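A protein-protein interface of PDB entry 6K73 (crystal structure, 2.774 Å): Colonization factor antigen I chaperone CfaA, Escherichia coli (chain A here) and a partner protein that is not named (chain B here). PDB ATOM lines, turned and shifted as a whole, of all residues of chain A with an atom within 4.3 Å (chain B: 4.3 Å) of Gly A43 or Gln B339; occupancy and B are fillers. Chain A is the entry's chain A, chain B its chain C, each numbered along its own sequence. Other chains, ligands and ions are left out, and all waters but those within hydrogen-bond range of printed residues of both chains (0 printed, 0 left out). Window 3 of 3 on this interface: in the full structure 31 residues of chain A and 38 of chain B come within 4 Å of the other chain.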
ATOM      1  N   ASN A  41      -1.698   9.091  10.210  1.00  0.00           N
ATOM      2  CA  ASN A  41      -2.962   8.869   9.518  1.00  0.00           C
ATOM      3  C   ASN A  41      -3.743   7.674  10.078  1.00  0.00           C
ATOM      4  O   ASN A  41      -4.173   6.802   9.320  1.00  0.00           O
ATOM      5  CB  ASN A  41      -2.724   8.691   8.024  1.00  0.00           C
ATOM      6  CG  ASN A  41      -2.035   9.894   7.390  1.00  0.00           C
ATOM      7  OD1 ASN A  41      -2.342  11.042   7.693  1.00  0.00           O
ATOM      8  ND2 ASN A  41      -1.085   9.620   6.493  1.00  0.00           N
ATOM      9  N   PRO A  42      -3.963   7.616  11.397  1.00  0.00           N
ATOM     10  CA  PRO A  42      -4.651   6.452  11.968  1.00  0.00           C
ATOM     11  C   PRO A  42      -6.113   6.395  11.540  1.00  0.00           C
ATOM     12  O   PRO A  42      -6.729   7.401  11.183  1.00  0.00           O
ATOM     13  CB  PRO A  42      -4.518   6.665  13.479  1.00  0.00           C
ATOM     14  CG  PRO A  42      -4.434   8.136  13.634  1.00  0.00           C
ATOM     15  CD  PRO A  42      -3.697   8.643  12.419  1.00  0.00           C
ATOM     16  N   GLY A  43      -6.665   5.179  11.571  1.00  0.00           N
ATOM     17  CA  GLY A  43      -8.026   4.933  11.119  1.00  0.00           C
ATOM     18  C   GLY A  43      -8.234   4.964   9.624  1.00  0.00           C
ATOM     19  O   GLY A  43      -9.328   4.622   9.167  1.00  0.00           O
ATOM     20  N   THR A  44      -7.228   5.345   8.843  1.00  0.00           N
ATOM     21  CA  THR A  44      -7.361   5.509   7.403  1.00  0.00           C
ATOM     22  C   THR A  44      -6.696   4.345   6.673  1.00  0.00           C
ATOM     23  O   THR A  44      -6.196   3.394   7.283  1.00  0.00           O
ATOM     24  CB  THR A  44      -6.759   6.848   6.965  1.00  0.00           C
ATOM     25  OG1 THR A  44      -5.366   6.878   7.297  1.00  0.00           O
ATOM     26  CG2 THR A  44      -7.467   8.010   7.649  1.00  0.00           C
ATOM     27  N   GLU A  47      -2.518   4.647   6.666  1.00  0.00           N
ATOM     28  CA  GLU A  47      -1.933   4.660   7.997  1.00  0.00           C
ATOM     29  C   GLU A  47      -0.560   4.005   7.982  1.00  0.00           C
ATOM     30  O   GLU A  47      -0.385   2.913   7.433  1.00  0.00           O
ATOM     31  CB  GLU A  47      -2.845   3.938   8.989  1.00  0.00           C
ATOM     32  CG  GLU A  47      -2.249   3.856  10.384  1.00  0.00           C
ATOM     33  CD  GLU A  47      -2.904   2.799  11.249  1.00  0.00           C
ATOM     34  OE1 GLU A  47      -4.128   2.874  11.465  1.00  0.00           O
ATOM     35  OE2 GLU A  47      -2.183   1.886  11.706  1.00  0.00           O
ATOM     36  N   ASN A 179     -19.018   1.071  12.002  1.00  0.00           N
ATOM     37  CA  ASN A 179     -18.072   0.551  12.984  1.00  0.00           C
ATOM     38  C   ASN A 179     -16.637   0.906  12.587  1.00  0.00           C
ATOM     39  O   ASN A 179     -15.769   0.047  12.441  1.00  0.00           O
ATOM     40  CB  ASN A 179     -18.242  -0.965  13.159  1.00  0.00           C
ATOM     41  CG  ASN A 179     -19.650  -1.354  13.588  1.00  0.00           C
ATOM     42  OD1 ASN A 179     -20.160  -0.883  14.607  1.00  0.00           O
ATOM     43  ND2 ASN A 179     -20.286  -2.218  12.805  1.00  0.00           N
ATOM     44  N   LYS A 180     -16.403   2.182  12.390  1.00  0.00           N
ATOM     45  CA  LYS A 180     -15.112   2.651  12.014  1.00  0.00           C
ATOM     46  C   LYS A 180     -14.867   3.906  12.797  1.00  0.00           C
ATOM     47  O   LYS A 180     -15.729   4.693  12.908  1.00  0.00           O
ATOM     48  CB  LYS A 180     -15.158   2.964  10.530  1.00  0.00           C
ATOM     49  CG  LYS A 180     -13.830   3.045   9.784  1.00  0.00           C
ATOM     50  CD  LYS A 180     -13.186   4.421   9.872  1.00  0.00           C
ATOM     51  CE  LYS A 180     -12.490   4.846   8.586  1.00  0.00           C
ATOM     52  NZ  LYS A 180     -11.914   6.222   8.593  1.00  0.00           N
ATOM     53  N   TYR A 183     -10.593   9.802  13.316  1.00  0.00           N
ATOM     54  CA  TYR A 183      -9.615  10.488  14.090  1.00  0.00           C
ATOM     55  C   TYR A 183      -9.589  11.949  13.772  1.00  0.00           C
ATOM     56  O   TYR A 183     -10.004  12.325  12.739  1.00  0.00           O
ATOM     57  CB  TYR A 183      -8.265   9.820  13.907  1.00  0.00           C
ATOM     58  CG  TYR A 183      -8.089   8.542  14.691  1.00  0.00           C
ATOM     59  CD1 TYR A 183      -8.609   7.367  14.251  1.00  0.00           C
ATOM     60  CD2 TYR A 183      -7.416   8.521  15.866  1.00  0.00           C
ATOM     61  CE1 TYR A 183      -8.470   6.217  14.970  1.00  0.00           C
ATOM     62  CE2 TYR A 183      -7.258   7.368  16.561  1.00  0.00           C
ATOM     63  CZ  TYR A 183      -7.789   6.232  16.099  1.00  0.00           C
ATOM     64  OH  TYR A 183      -7.653   5.102  16.812  1.00  0.00           O
ATOM     65  N   SER B 337      -6.049  -2.766  16.369  1.00  0.00           N
ATOM     66  CA  SER B 337      -5.918  -1.881  15.224  1.00  0.00           C
ATOM     67  C   SER B 337      -6.662  -0.572  15.474  1.00  0.00           C
ATOM     68  O   SER B 337      -7.437  -0.437  16.426  1.00  0.00           O
ATOM     69  CB  SER B 337      -6.403  -2.556  13.938  1.00  0.00           C
ATOM     70  OG  SER B 337      -7.672  -3.152  14.093  1.00  0.00           O
ATOM     71  N   SER B 338      -6.396   0.402  14.605  1.00  0.00           N
ATOM     72  CA  SER B 338      -6.975   1.731  14.721  1.00  0.00           C
ATOM     73  C   SER B 338      -8.383   1.822  14.137  1.00  0.00           C
ATOM     74  O   SER B 338      -9.213   2.570  14.667  1.00  0.00           O
ATOM     75  CB  SER B 338      -6.071   2.753  14.018  1.00  0.00           C
ATOM     76  OG  SER B 338      -4.770   2.230  13.798  1.00  0.00           O
ATOM     77  N   GLN B 339      -8.674   1.067  13.075  1.00  0.00           N
ATOM     78  CA  GLN B 339     -10.000   1.064  12.466  1.00  0.00           C
ATOM     79  C   GLN B 339     -10.998   0.250  13.290  1.00  0.00           C
ATOM     80  O   GLN B 339     -11.772  -0.541  12.738  1.00  0.00           O
ATOM     81  CB  GLN B 339      -9.922   0.521  11.037  1.00  0.00           C
ATOM     82  CG  GLN B 339      -9.115   1.379  10.060  1.00  0.00           C
ATOM     83  CD  GLN B 339      -7.642   1.010  10.004  1.00  0.00           C
ATOM     84  OE1 GLN B 339      -6.975   0.897  11.033  1.00  0.00           O
ATOM     85  NE2 GLN B 339      -7.127   0.827   8.794  1.00  0.00           N
ATOM     86  N   THR B 340     -10.976   0.447  14.605  1.00  0.00           N
ATOM     87  CA  THR B 340     -11.877  -0.268  15.501  1.00  0.00           C
ATOM     88  C   THR B 340     -12.810   0.697  16.228  1.00  0.00           C
ATOM     89  O   THR B 340     -12.907   1.870  15.869  1.00  0.00           O
ATOM     90  CB  THR B 340     -11.101  -1.096  16.539  1.00  0.00           C
ATOM     91  OG1 THR B 340     -10.282  -0.228  17.333  1.00  0.00           O
ATOM     92  CG2 THR B 340     -10.219  -2.125  15.848  1.00  0.00           C
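The side-chain carboxylate of Glu A47 is in hydrogen-bond range of the backbone NH of Gly A43. O of Gly A43 is in hydrogen-bond range of NZ of Lys A180.
The side-chain amide nitrogen of Gln B339 is in hydrogen-bond range of the backbone carbonyl oxygen of Thr A44 (3.1 Å). OG of Ser B338 lies within hydrogen-bond range of OE1 of Glu A47. OE1 of Glu A47 lies close to OE1 of Gln B339 (3.5 Å).
Among the printed residues, pairs that only touch across the chains: Gly A43 with Gln B339 (3.4 Å), Gly A43 with Ser B338 (3.5 Å) and Tyr A183 with Ser B338 (3.7 Å).
Gly A43 touches just these residues of chain B: Ser B338 and Gln B339. Gln B339 touches three residues of chain A. Printed residues of chain B within 4 Å of Glu A47: Ser B338 and Gln B339. Of the printed residues of chain B, Tyr A183 touches Ser B338. Of the printed residues of chain B, Thr A44 touches Gln B339 (3.1 Å). Of the printed residues of chain A, Ser B338 touches Gly A43, Glu A47 and Tyr A183. Thr B340 touches none of the printed residues of chain A. Asn A41 touches none of the printed residues of chain B. The nearest printed residue of chain B that does not touch Thr A44 is Ser B338 (5.9 Å).
Of the 4 printed residues of chain B, 2 touch a printed residue of chain A. Hydrophobic or aromatic side chains of chain A that line the printed part of chain B: Tyr A183. Among the printed residues, no Asp or Glu carboxylate lies within 4 Å of a Lys or Arg side-chain nitrogen of the other chain.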
